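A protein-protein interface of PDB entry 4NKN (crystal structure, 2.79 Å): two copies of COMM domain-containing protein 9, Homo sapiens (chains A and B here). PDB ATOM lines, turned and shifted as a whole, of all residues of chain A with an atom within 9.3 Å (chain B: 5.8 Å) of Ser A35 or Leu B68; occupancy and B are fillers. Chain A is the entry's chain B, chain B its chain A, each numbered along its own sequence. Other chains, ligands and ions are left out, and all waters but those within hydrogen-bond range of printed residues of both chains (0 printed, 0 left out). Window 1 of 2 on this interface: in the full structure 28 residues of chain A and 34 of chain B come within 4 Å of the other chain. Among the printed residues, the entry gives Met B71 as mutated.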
ATOM      1  N   LEU A   8      16.556  25.569 -14.196  1.00  0.00           N
ATOM      2  CA  LEU A   8      16.377  25.631 -15.642  1.00  0.00           C
ATOM      3  C   LEU A   8      14.928  25.917 -16.017  1.00  0.00           C
ATOM      4  O   LEU A   8      14.018  25.179 -15.643  1.00  0.00           O
ATOM      5  CB  LEU A   8      16.843  24.327 -16.288  1.00  0.00           C
ATOM      6  CG  LEU A   8      18.352  24.087 -16.225  1.00  0.00           C
ATOM      7  CD1 LEU A   8      18.684  22.657 -16.604  1.00  0.00           C
ATOM      8  CD2 LEU A   8      19.083  25.062 -17.133  1.00  0.00           C
ATOM      9  N   GLU A  11      11.944  27.992 -21.162  1.00  0.00           N
ATOM     10  CA  GLU A  11      12.573  28.597 -22.333  1.00  0.00           C
ATOM     11  C   GLU A  11      13.913  27.938 -22.641  1.00  0.00           C
ATOM     12  O   GLU A  11      14.316  27.841 -23.801  1.00  0.00           O
ATOM     13  CB  GLU A  11      12.772  30.102 -22.131  1.00  0.00           C
ATOM     14  CG  GLU A  11      11.487  30.907 -22.024  1.00  0.00           C
ATOM     15  CD  GLU A  11      10.945  30.962 -20.608  1.00  0.00           C
ATOM     16  OE1 GLU A  11      11.753  31.089 -19.663  1.00  0.00           O
ATOM     17  OE2 GLU A  11       9.709  30.878 -20.441  1.00  0.00           O
ATOM     18  N   HIS A  12      14.602  27.493 -21.595  1.00  0.00           N
ATOM     19  CA  HIS A  12      15.896  26.835 -21.744  1.00  0.00           C
ATOM     20  C   HIS A  12      15.773  25.505 -22.480  1.00  0.00           C
ATOM     21  O   HIS A  12      16.546  25.218 -23.394  1.00  0.00           O
ATOM     22  CB  HIS A  12      16.541  26.613 -20.375  1.00  0.00           C
ATOM     23  CG  HIS A  12      17.074  27.863 -19.748  1.00  0.00           C
ATOM     24  ND1 HIS A  12      17.031  28.091 -18.388  1.00  0.00           N
ATOM     25  CD2 HIS A  12      17.670  28.949 -20.292  1.00  0.00           C
ATOM     26  CE1 HIS A  12      17.571  29.266 -18.124  1.00  0.00           C
ATOM     27  NE2 HIS A  12      17.970  29.807 -19.262  1.00  0.00           N
ATOM     28  N   PHE A  13      14.799  24.697 -22.073  1.00  0.00           N
ATOM     29  CA  PHE A  13      14.584  23.390 -22.681  1.00  0.00           C
ATOM     30  C   PHE A  13      14.077  23.515 -24.112  1.00  0.00           C
ATOM     31  O   PHE A  13      14.296  22.630 -24.937  1.00  0.00           O
ATOM     32  CB  PHE A  13      13.601  22.568 -21.846  1.00  0.00           C
ATOM     33  CG  PHE A  13      14.158  22.118 -20.530  1.00  0.00           C
ATOM     34  CD1 PHE A  13      15.166  21.171 -20.482  1.00  0.00           C
ATOM     35  CD2 PHE A  13      13.675  22.638 -19.341  1.00  0.00           C
ATOM     36  CE1 PHE A  13      15.687  20.752 -19.275  1.00  0.00           C
ATOM     37  CE2 PHE A  13      14.190  22.222 -18.128  1.00  0.00           C
ATOM     38  CZ  PHE A  13      15.198  21.277 -18.095  1.00  0.00           C
ATOM     39  N   ALA A  15      15.101  25.920 -26.044  1.00  0.00           N
ATOM     40  CA  ALA A  15      16.297  26.346 -26.759  1.00  0.00           C
ATOM     41  C   ALA A  15      17.226  25.167 -27.039  1.00  0.00           C
ATOM     42  O   ALA A  15      17.891  25.122 -28.075  1.00  0.00           O
ATOM     43  CB  ALA A  15      17.026  27.421 -25.967  1.00  0.00           C
ATOM     44  N   LEU A  16      17.261  24.215 -26.110  1.00  0.00           N
ATOM     45  CA  LEU A  16      18.122  23.040 -26.229  1.00  0.00           C
ATOM     46  C   LEU A  16      17.750  22.169 -27.421  1.00  0.00           C
ATOM     47  O   LEU A  16      18.610  21.530 -28.027  1.00  0.00           O
ATOM     48  CB  LEU A  16      18.057  22.204 -24.951  1.00  0.00           C
ATOM     49  CG  LEU A  16      18.738  22.786 -23.714  1.00  0.00           C
ATOM     50  CD1 LEU A  16      18.484  21.901 -22.508  1.00  0.00           C
ATOM     51  CD2 LEU A  16      20.226  22.944 -23.960  1.00  0.00           C
ATOM     52  N   GLN A  17      16.465  22.152 -27.754  1.00  0.00           N
ATOM     53  CA  GLN A  17      15.953  21.280 -28.807  1.00  0.00           C
ATOM     54  C   GLN A  17      16.462  21.671 -30.189  1.00  0.00           C
ATOM     55  O   GLN A  17      16.339  20.901 -31.138  1.00  0.00           O
ATOM     56  CB  GLN A  17      14.424  21.283 -28.793  1.00  0.00           C
ATOM     57  CG  GLN A  17      13.830  20.792 -27.486  1.00  0.00           C
ATOM     58  CD  GLN A  17      12.340  21.046 -27.382  1.00  0.00           C
ATOM     59  OE1 GLN A  17      11.688  21.403 -28.361  1.00  0.00           O
ATOM     60  NE2 GLN A  17      11.794  20.861 -26.188  1.00  0.00           N
ATOM     61  N   SER A  18      17.042  22.864 -30.294  1.00  0.00           N
ATOM     62  CA  SER A  18      17.623  23.328 -31.550  1.00  0.00           C
ATOM     63  C   SER A  18      18.797  22.452 -31.984  1.00  0.00           C
ATOM     64  O   SER A  18      19.175  22.441 -33.156  1.00  0.00           O
ATOM     65  CB  SER A  18      18.077  24.785 -31.428  1.00  0.00           C
ATOM     66  OG  SER A  18      16.976  25.649 -31.208  1.00  0.00           O
ATOM     67  N   LEU A  19      19.362  21.713 -31.033  1.00  0.00           N
ATOM     68  CA  LEU A  19      20.493  20.826 -31.297  1.00  0.00           C
ATOM     69  C   LEU A  19      20.126  19.697 -32.255  1.00  0.00           C
ATOM     70  O   LEU A  19      21.001  19.001 -32.772  1.00  0.00           O
ATOM     71  CB  LEU A  19      21.028  20.244 -29.986  1.00  0.00           C
ATOM     72  CG  LEU A  19      21.694  21.229 -29.023  1.00  0.00           C
ATOM     73  CD1 LEU A  19      21.917  20.585 -27.666  1.00  0.00           C
ATOM     74  CD2 LEU A  19      23.008  21.738 -29.593  1.00  0.00           C
ATOM     75  N   VAL A  27      29.145  18.025 -33.295  1.00  0.00           N
ATOM     76  CA  VAL A  27      28.814  19.441 -33.173  1.00  0.00           C
ATOM     77  C   VAL A  27      28.114  19.706 -31.846  1.00  0.00           C
ATOM     78  O   VAL A  27      28.410  20.680 -31.153  1.00  0.00           O
ATOM     79  CB  VAL A  27      27.913  19.918 -34.325  1.00  0.00           C
ATOM     80  CG1 VAL A  27      27.643  21.408 -34.199  1.00  0.00           C
ATOM     81  CG2 VAL A  27      28.548  19.596 -35.669  1.00  0.00           C
ATOM     82  N   VAL A  28      27.182  18.822 -31.506  1.00  0.00           N
ATOM     83  CA  VAL A  28      26.468  18.886 -30.238  1.00  0.00           C
ATOM     84  C   VAL A  28      27.447  18.785 -29.071  1.00  0.00           C
ATOM     85  O   VAL A  28      27.299  19.470 -28.059  1.00  0.00           O
ATOM     86  CB  VAL A  28      25.419  17.763 -30.137  1.00  0.00           C
ATOM     87  CG1 VAL A  28      24.677  17.834 -28.813  1.00  0.00           C
ATOM     88  CG2 VAL A  28      24.447  17.842 -31.308  1.00  0.00           C
ATOM     89  N   ARG A  29      28.455  17.933 -29.230  1.00  0.00           N
ATOM     90  CA  ARG A  29      29.473  17.743 -28.203  1.00  0.00           C
ATOM     91  C   ARG A  29      30.347  18.984 -28.052  1.00  0.00           C
ATOM     92  O   ARG A  29      30.704  19.369 -26.939  1.00  0.00           O
ATOM     93  CB  ARG A  29      30.339  16.526 -28.532  1.00  0.00           C
ATOM     94  CG  ARG A  29      31.199  16.040 -27.377  1.00  0.00           C
ATOM     95  CD  ARG A  29      32.009  14.819 -27.777  1.00  0.00           C
ATOM     96  NE  ARG A  29      31.191  13.836 -28.482  1.00  0.00           N
ATOM     97  CZ  ARG A  29      30.489  12.877 -27.886  1.00  0.00           C
ATOM     98  NH1 ARG A  29      30.501  12.765 -26.564  1.00  0.00           N
ATOM     99  NH2 ARG A  29      29.774  12.029 -28.613  1.00  0.00           N
ATOM    100  N   GLN A  30      30.689  19.604 -29.177  1.00  0.00           N
ATOM    101  CA  GLN A  30      31.522  20.802 -29.169  1.00  0.00           C
ATOM    102  C   GLN A  30      30.801  21.975 -28.516  1.00  0.00           C
ATOM    103  O   GLN A  30      31.379  22.693 -27.699  1.00  0.00           O
ATOM    104  CB  GLN A  30      31.935  21.182 -30.590  1.00  0.00           C
ATOM    105  CG  GLN A  30      32.736  22.473 -30.668  1.00  0.00           C
ATOM    106  CD  GLN A  30      32.795  23.045 -32.070  1.00  0.00           C
ATOM    107  OE1 GLN A  30      32.151  22.537 -32.988  1.00  0.00           O
ATOM    108  NE2 GLN A  30      33.568  24.111 -32.241  1.00  0.00           N
ATOM    109  N   LEU A  31      29.537  22.161 -28.882  1.00  0.00           N
ATOM    110  CA  LEU A  31      28.734  23.267 -28.370  1.00  0.00           C
ATOM    111  C   LEU A  31      28.560  23.201 -26.856  1.00  0.00           C
ATOM    112  O   LEU A  31      28.450  24.232 -26.196  1.00  0.00           O
ATOM    113  CB  LEU A  31      27.364  23.289 -29.053  1.00  0.00           C
ATOM    114  CG  LEU A  31      27.358  23.753 -30.510  1.00  0.00           C
ATOM    115  CD1 LEU A  31      25.992  23.546 -31.147  1.00  0.00           C
ATOM    116  CD2 LEU A  31      27.778  25.212 -30.605  1.00  0.00           C
ATOM    117  N   CYS A  32      28.537  21.989 -26.311  1.00  0.00           N
ATOM    118  CA  CYS A  32      28.411  21.802 -24.870  1.00  0.00           C
ATOM    119  C   CYS A  32      29.685  22.229 -24.152  1.00  0.00           C
ATOM    120  O   CYS A  32      29.636  22.947 -23.153  1.00  0.00           O
ATOM    121  CB  CYS A  32      28.082  20.343 -24.541  1.00  0.00           C
ATOM    122  SG  CYS A  32      26.418  19.821 -25.018  1.00  0.00           S
ATOM    123  N   GLN A  33      30.825  21.784 -24.674  1.00  0.00           N
ATOM    124  CA  GLN A  33      32.124  22.122 -24.103  1.00  0.00           C
ATOM    125  C   GLN A  33      32.383  23.625 -24.163  1.00  0.00           C
ATOM    126  O   GLN A  33      32.842  24.226 -23.193  1.00  0.00           O
ATOM    127  CB  GLN A  33      33.242  21.376 -24.835  1.00  0.00           C
ATOM    128  CG  GLN A  33      33.146  19.861 -24.762  1.00  0.00           C
ATOM    129  CD  GLN A  33      34.138  19.173 -25.681  1.00  0.00           C
ATOM    130  OE1 GLN A  33      34.378  19.624 -26.802  1.00  0.00           O
ATOM    131  NE2 GLN A  33      34.726  18.081 -25.207  1.00  0.00           N
ATOM    132  N   GLU A  34      32.080  24.222 -25.312  1.00  0.00           N
ATOM    133  CA  GLU A  34      32.319  25.645 -25.529  1.00  0.00           C
ATOM    134  C   GLU A  34      31.384  26.519 -24.698  1.00  0.00           C
ATOM    135  O   GLU A  34      31.750  27.624 -24.299  1.00  0.00           O
ATOM    136  CB  GLU A  34      32.173  25.989 -27.011  1.00  0.00           C
ATOM    137  CG  GLU A  34      33.244  25.377 -27.904  1.00  0.00           C
ATOM    138  CD  GLU A  34      34.641  25.852 -27.553  1.00  0.00           C
ATOM    139  OE1 GLU A  34      35.036  26.942 -28.016  1.00  0.00           O
ATOM    140  OE2 GLU A  34      35.344  25.133 -26.812  1.00  0.00           O
ATOM    141  N   SER A  35      30.177  26.022 -24.439  1.00  0.00           N
ATOM    142  CA  SER A  35      29.200  26.766 -23.650  1.00  0.00           C
ATOM    143  C   SER A  35      29.587  26.818 -22.180  1.00  0.00           C
ATOM    144  O   SER A  35      29.381  27.829 -21.510  1.00  0.00           O
ATOM    145  CB  SER A  35      27.810  26.150 -23.795  1.00  0.00           C
ATOM    146  OG  SER A  35      27.317  26.314 -25.113  1.00  0.00           O
ATOM    147  N   PHE A  36      30.141  25.718 -21.680  1.00  0.00           N
ATOM    148  CA  PHE A  36      30.577  25.655 -20.292  1.00  0.00           C
ATOM    149  C   PHE A  36      31.754  26.592 -20.060  1.00  0.00           C
ATOM    150  O   PHE A  36      31.809  27.298 -19.054  1.00  0.00           O
ATOM    151  CB  PHE A  36      30.962  24.221 -19.909  1.00  0.00           C
ATOM    152  CG  PHE A  36      31.376  24.066 -18.470  1.00  0.00           C
ATOM    153  CD1 PHE A  36      30.438  23.775 -17.494  1.00  0.00           C
ATOM    154  CD2 PHE A  36      32.704  24.211 -18.093  1.00  0.00           C
ATOM    155  CE1 PHE A  36      30.812  23.630 -16.171  1.00  0.00           C
ATOM    156  CE2 PHE A  36      33.083  24.071 -16.769  1.00  0.00           C
ATOM    157  CZ  PHE A  36      32.135  23.781 -15.808  1.00  0.00           C
ATOM    158  N   SER A  37      32.690  26.596 -21.003  1.00  0.00           N
ATOM    159  CA  SER A  37      33.929  27.351 -20.856  1.00  0.00           C
ATOM    160  C   SER A  37      33.755  28.837 -21.160  1.00  0.00           C
ATOM    161  O   SER A  37      34.591  29.655 -20.776  1.00  0.00           O
ATOM    162  CB  SER A  37      35.013  26.762 -21.762  1.00  0.00           C
ATOM    163  OG  SER A  37      35.225  25.391 -21.478  1.00  0.00           O
ATOM    164  N   SER A  38      32.672  29.184 -21.847  1.00  0.00           N
ATOM    165  CA  SER A  38      32.420  30.573 -22.218  1.00  0.00           C
ATOM    166  C   SER A  38      32.080  31.434 -21.005  1.00  0.00           C
ATOM    167  O   SER A  38      30.960  31.389 -20.493  1.00  0.00           O
ATOM    168  CB  SER A  38      31.288  30.659 -23.243  1.00  0.00           C
ATOM    169  OG  SER A  38      31.035  32.005 -23.608  1.00  0.00           O
ATOM    170  N   SER A  39      33.051  32.220 -20.553  1.00  0.00           N
ATOM    171  CA  SER A  39      32.859  33.095 -19.403  1.00  0.00           C
ATOM    172  C   SER A  39      31.878  34.222 -19.708  1.00  0.00           C
ATOM    173  O   SER A  39      31.189  34.717 -18.816  1.00  0.00           O
ATOM    174  CB  SER A  39      34.199  33.680 -18.950  1.00  0.00           C
ATOM    175  OG  SER A  39      34.014  34.642 -17.925  1.00  0.00           O
ATOM    176  N   ALA A  40      31.820  34.621 -20.973  1.00  0.00           N
ATOM    177  CA  ALA A  40      30.976  35.736 -21.386  1.00  0.00           C
ATOM    178  C   ALA A  40      29.492  35.379 -21.337  1.00  0.00           C
ATOM    179  O   ALA A  40      28.641  36.260 -21.227  1.00  0.00           O
ATOM    180  CB  ALA A  40      31.362  36.198 -22.781  1.00  0.00           C
ATOM    181  N   LEU A  41      29.187  34.086 -21.417  1.00  0.00           N
ATOM    182  CA  LEU A  41      27.802  33.624 -21.403  1.00  0.00           C
ATOM    183  C   LEU A  41      27.134  33.848 -20.051  1.00  0.00           C
ATOM    184  O   LEU A  41      25.920  34.033 -19.974  1.00  0.00           O
ATOM    185  CB  LEU A  41      27.727  32.141 -21.776  1.00  0.00           C
ATOM    186  CG  LEU A  41      27.728  31.818 -23.270  1.00  0.00           C
ATOM    187  CD1 LEU A  41      27.668  30.316 -23.497  1.00  0.00           C
ATOM    188  CD2 LEU A  41      26.563  32.513 -23.958  1.00  0.00           C
ATOM    189  N   GLY A  42      27.930  33.836 -18.987  1.00  0.00           N
ATOM    190  CA  GLY A  42      27.411  34.046 -17.647  1.00  0.00           C
ATOM    191  C   GLY A  42      27.094  35.503 -17.370  1.00  0.00           C
ATOM    192  O   GLY A  42      27.529  36.061 -16.362  1.00  0.00           O
ATOM    193  N   LEU B  46      31.896  31.846 -31.328  1.00  0.00           N
ATOM    194  CA  LEU B  46      31.104  30.663 -31.015  1.00  0.00           C
ATOM    195  C   LEU B  46      29.685  30.791 -31.559  1.00  0.00           C
ATOM    196  O   LEU B  46      29.084  29.809 -31.992  1.00  0.00           O
ATOM    197  CB  LEU B  46      31.074  30.429 -29.502  1.00  0.00           C
ATOM    198  CG  LEU B  46      30.244  29.241 -29.012  1.00  0.00           C
ATOM    199  CD1 LEU B  46      30.678  27.960 -29.708  1.00  0.00           C
ATOM    200  CD2 LEU B  46      30.348  29.102 -27.501  1.00  0.00           C
ATOM    201  N   GLU B  63      20.255  31.890 -27.379  1.00  0.00           N
ATOM    202  CA  GLU B  63      19.410  31.204 -26.408  1.00  0.00           C
ATOM    203  C   GLU B  63      19.949  29.817 -26.080  1.00  0.00           C
ATOM    204  O   GLU B  63      20.013  29.428 -24.914  1.00  0.00           O
ATOM    205  CB  GLU B  63      17.975  31.092 -26.928  1.00  0.00           C
ATOM    206  CG  GLU B  63      17.274  32.424 -27.112  1.00  0.00           C
ATOM    207  CD  GLU B  63      15.887  32.272 -27.710  1.00  0.00           C
ATOM    208  OE1 GLU B  63      15.234  33.307 -27.970  1.00  0.00           O
ATOM    209  OE2 GLU B  63      15.451  31.119 -27.918  1.00  0.00           O
ATOM    210  N   LEU B  64      20.333  29.080 -27.117  1.00  0.00           N
ATOM    211  CA  LEU B  64      20.860  27.729 -26.955  1.00  0.00           C
ATOM    212  C   LEU B  64      22.148  27.711 -26.139  1.00  0.00           C
ATOM    213  O   LEU B  64      22.321  26.874 -25.253  1.00  0.00           O
ATOM    214  CB  LEU B  64      21.104  27.084 -28.320  1.00  0.00           C
ATOM    215  CG  LEU B  64      21.896  25.774 -28.321  1.00  0.00           C
ATOM    216  CD1 LEU B  64      21.185  24.694 -27.519  1.00  0.00           C
ATOM    217  CD2 LEU B  64      22.141  25.310 -29.741  1.00  0.00           C
ATOM    218  N   LEU B  65      23.050  28.639 -26.442  1.00  0.00           N
ATOM    219  CA  LEU B  65      24.327  28.715 -25.745  1.00  0.00           C
ATOM    220  C   LEU B  65      24.138  29.103 -24.282  1.00  0.00           C
ATOM    221  O   LEU B  65      24.829  28.587 -23.406  1.00  0.00           O
ATOM    222  CB  LEU B  65      25.260  29.705 -26.444  1.00  0.00           C
ATOM    223  CG  LEU B  65      25.672  29.307 -27.864  1.00  0.00           C
ATOM    224  CD1 LEU B  65      26.718  30.263 -28.414  1.00  0.00           C
ATOM    225  CD2 LEU B  65      26.176  27.870 -27.894  1.00  0.00           C
ATOM    226  N   GLN B  66      23.198  30.008 -24.022  1.00  0.00           N
ATOM    227  CA  GLN B  66      22.851  30.371 -22.653  1.00  0.00           C
ATOM    228  C   GLN B  66      22.212  29.183 -21.944  1.00  0.00           C
ATOM    229  O   GLN B  66      22.415  28.978 -20.746  1.00  0.00           O
ATOM    230  CB  GLN B  66      21.905  31.572 -22.624  1.00  0.00           C
ATOM    231  CG  GLN B  66      22.551  32.889 -23.025  1.00  0.00           C
ATOM    232  N   ALA B  67      21.441  28.404 -22.694  1.00  0.00           N
ATOM    233  CA  ALA B  67      20.809  27.206 -22.155  1.00  0.00           C
ATOM    234  C   ALA B  67      21.862  26.165 -21.796  1.00  0.00           C
ATOM    235  O   ALA B  67      21.894  25.662 -20.672  1.00  0.00           O
ATOM    236  CB  ALA B  67      19.813  26.632 -23.151  1.00  0.00           C
ATOM    237  N   LEU B  68      22.722  25.850 -22.760  1.00  0.00           N
ATOM    238  CA  LEU B  68      23.797  24.890 -22.550  1.00  0.00           C
ATOM    239  C   LEU B  68      24.747  25.340 -21.447  1.00  0.00           C
ATOM    240  O   LEU B  68      25.274  24.516 -20.704  1.00  0.00           O
ATOM    241  CB  LEU B  68      24.578  24.664 -23.847  1.00  0.00           C
ATOM    242  CG  LEU B  68      23.946  23.745 -24.894  1.00  0.00           C
ATOM    243  CD1 LEU B  68      24.772  23.748 -26.173  1.00  0.00           C
ATOM    244  CD2 LEU B  68      23.807  22.330 -24.351  1.00  0.00           C
ATOM    245  N   HIS B  69      24.963  26.647 -21.339  1.00  0.00           N
ATOM    246  CA  HIS B  69      25.863  27.172 -20.319  1.00  0.00           C
ATOM    247  C   HIS B  69      25.311  26.937 -18.917  1.00  0.00           C
ATOM    248  O   HIS B  69      26.036  26.504 -18.023  1.00  0.00           O
ATOM    249  CB  HIS B  69      26.118  28.665 -20.533  1.00  0.00           C
ATOM    250  CG  HIS B  69      27.051  29.266 -19.527  1.00  0.00           C
ATOM    251  ND1 HIS B  69      28.405  29.013 -19.524  1.00  0.00           N
ATOM    252  CD2 HIS B  69      26.823  30.107 -18.491  1.00  0.00           C
ATOM    253  CE1 HIS B  69      28.973  29.674 -18.529  1.00  0.00           C
ATOM    254  NE2 HIS B  69      28.034  30.345 -17.888  1.00  0.00           N
ATOM    255  N   ARG B  70      24.025  27.220 -18.733  1.00  0.00           N
ATOM    256  CA  ARG B  70      23.405  27.083 -17.422  1.00  0.00           C
ATOM    257  C   ARG B  70      23.276  25.619 -17.018  1.00  0.00           C
ATOM    258  O   ARG B  70      23.416  25.280 -15.846  1.00  0.00           O
ATOM    259  CB  ARG B  70      22.034  27.764 -17.399  1.00  0.00           C
ATOM    260  CG  ARG B  70      21.361  27.755 -16.034  1.00  0.00           C
ATOM    261  CD  ARG B  70      20.157  28.680 -16.000  1.00  0.00           C
ATOM    262  NE  ARG B  70      20.532  30.080 -16.182  1.00  0.00           N
ATOM    263  N   MET B  71      23.024  24.749 -17.992  1.00  0.00           N
ATOM    264  CA  MET B  71      22.853  23.327 -17.705  1.00  0.00           C
ATOM    265  C   MET B  71      24.177  22.652 -17.352  1.00  0.00           C
ATOM    266  O   MET B  71      24.271  21.949 -16.346  1.00  0.00           O
ATOM    267  CB  MET B  71      22.205  22.607 -18.890  1.00  0.00           C
ATOM    268  CG  MET B  71      22.167  21.093 -18.734  1.00  0.00           C
ATOM    269  SD  MET B  71      21.112  20.173 -20.094  1.00  0.00           S
ATOM    270  CE  MET B  71      19.356  20.302 -19.264  1.00  0.00           C
ATOM    271  N   THR B  72      25.195  22.871 -18.176  1.00  0.00           N
ATOM    272  CA  THR B  72      26.498  22.243 -17.969  1.00  0.00           C
ATOM    273  C   THR B  72      27.143  22.710 -16.668  1.00  0.00           C
ATOM    274  O   THR B  72      27.796  21.930 -15.974  1.00  0.00           O
ATOM    275  CB  THR B  72      27.455  22.527 -19.141  1.00  0.00           C
ATOM    276  OG1 THR B  72      27.534  23.940 -19.364  1.00  0.00           O
ATOM    277  CG2 THR B  72      26.960  21.845 -20.410  1.00  0.00           C
ATOM    278  N   ARG B  73      26.959  23.986 -16.343  1.00  0.00           N
ATOM    279  CA  ARG B  73      27.431  24.526 -15.073  1.00  0.00           C
ATOM    280  C   ARG B  73      26.655  23.916 -13.913  1.00  0.00           C
ATOM    281  O   ARG B  73      27.223  23.617 -12.863  1.00  0.00           O
ATOM    282  CB  ARG B  73      27.299  26.051 -15.050  1.00  0.00           C
ATOM    283  CG  ARG B  73      28.341  26.785 -15.877  1.00  0.00           C
ATOM    284  CD  ARG B  73      29.694  26.793 -15.185  1.00  0.00           C
ATOM    285  NE  ARG B  73      30.728  27.402 -16.018  1.00  0.00           N
ATOM    286  CZ  ARG B  73      31.982  27.603 -15.627  1.00  0.00           C
ATOM    287  NH1 ARG B  73      32.366  27.243 -14.409  1.00  0.00           N
ATOM    288  NH2 ARG B  73      32.853  28.163 -16.453  1.00  0.00           N
ATOM    289  N   LEU B 102      22.530  14.258 -24.823  1.00  0.00           N
ATOM    290  CA  LEU B 102      22.993  15.302 -23.918  1.00  0.00           C
ATOM    291  C   LEU B 102      23.426  14.744 -22.563  1.00  0.00           C
ATOM    292  O   LEU B 102      24.432  15.180 -22.005  1.00  0.00           O
ATOM    293  CB  LEU B 102      21.904  16.359 -23.725  1.00  0.00           C
ATOM    294  CG  LEU B 102      21.681  17.297 -24.914  1.00  0.00           C
ATOM    295  CD1 LEU B 102      20.521  18.246 -24.657  1.00  0.00           C
ATOM    296  CD2 LEU B 102      22.951  18.071 -25.206  1.00  0.00           C
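Of chain B, only Leu B65 (3.4 Å), Leu B68 (3.4 Å) and His B69 (2.5 Å) come within 4 Å of Ser A35. Leu B68 touches just these residues of chain A: Leu A16 (3.7 Å), Leu A31 (3.7 Å), Cys A32 (3.7 Å) and Ser A35 (3.4 Å). Leu B65 touches two residues of chain A. Printed residues of chain A within 4 Å of Ala B67: His A12 (3.6 Å) and Leu A16 (3.8 Å). Of chain A, only Ser A35 (2.5 Å), Phe A36 (3.7 Å), Ser A38 (3.3 Å), Leu A41 (3.7 Å) and Gly A42 (3.7 Å) come within 4 Å of His B69. Printed residues of chain B within 4 Å of Leu A41: Leu B65 and His B69. Of the printed residues of chain B, Leu A19 touches Leu B64 (3.7 Å) and Leu B102 (3.7 Å). Of the printed residues of chain A, Leu B102 touches Leu A19 and Cys A32. Gln A30 touches none of the printed residues of chain B. Val A28 touches none of the printed residues of chain B. The nearest residue of chain A that does not touch Leu B68 is Leu A19 (4.2 Å). The nearest printed residue of chain B that does not touch Cys A32 is His B69 (6.2 Å).
No position is printed for both chains. Of the 28 pairs that touch across the chains among the printed residues, none has its exchanged pair printed and touching as well.
Among the printed residues, pairs that only touch across the chains: Ser A38 with His B69, Leu A41 with Leu B65, Ala A15 with Leu B64, Ser A35 with Leu B65, His A12 with Arg B70, Ser A35 with Leu B68, Phe A36 with Thr B72, His A12 with Ala B67, Leu A8 with Met B71, Glu A34 with Leu B46, Leu A16 with Leu B68, Gly A42 with His B69, Leu A19 with Leu B102, Leu A19 with Leu B64, Cys A32 with Leu B68, Leu A8 with Arg B70, Phe A13 with Met B71, Leu A31 with Leu B68, Leu A41 with His B69, Leu A16 with Leu B64, Leu A16 with Met B71, Phe A36 with His B69, Ala A15 with Glu B63, Leu A16 with Ala B67, Cys A32 with Leu B102 and Cys A32 with Thr B72.
The backbone carbonyl oxygen of Leu B68 is in hydrogen-bond range of the side-chain hydroxyl of Thr B72 (2.7 Å). The backbone carbonyl oxygen (O) of His B69 sits at hydrogen-bond distance from the side-chain hydroxyl (OG1) of Thr B72, 3.3 Å away. The backbone carbonyl oxygen (O) of Phe A13 sits close to the side-chain amide nitrogen (NE2) of Gln A17. O of Ala A15 sits at hydrogen-bond distance from OG of Ser A18. The backbone carbonyl oxygen (O) of Val A28 sits at hydrogen-bond distance from the side-chain sulfur (SG) of Cys A32 (3.2 Å). O of Leu A31 lies within hydrogen-bond range of OG of Ser A35, 2.6 Å away.
ND1 of His B69 sits at hydrogen-bond distance from O of Ser A35 (2.5 Å). The backbone carbonyl oxygen of Phe A36 is in hydrogen-bond range of the guanidinium group of Arg B73, 2.9 Å away.
Of the 25 printed residues of chain A, 14 touch a printed residue of chain B. Hydrophobic or aromatic side chains of chain A within 4 Å of the printed part of chain B: Leu A8, His A12, Phe A13, Ala A15, Leu A16, Leu A19, Leu A31, Phe A36 and Leu A41. Along chain B the printed residues that touch a printed residue of chain A span positions 46 to 102. Among the printed residues, 28 pairs touch across the chains.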
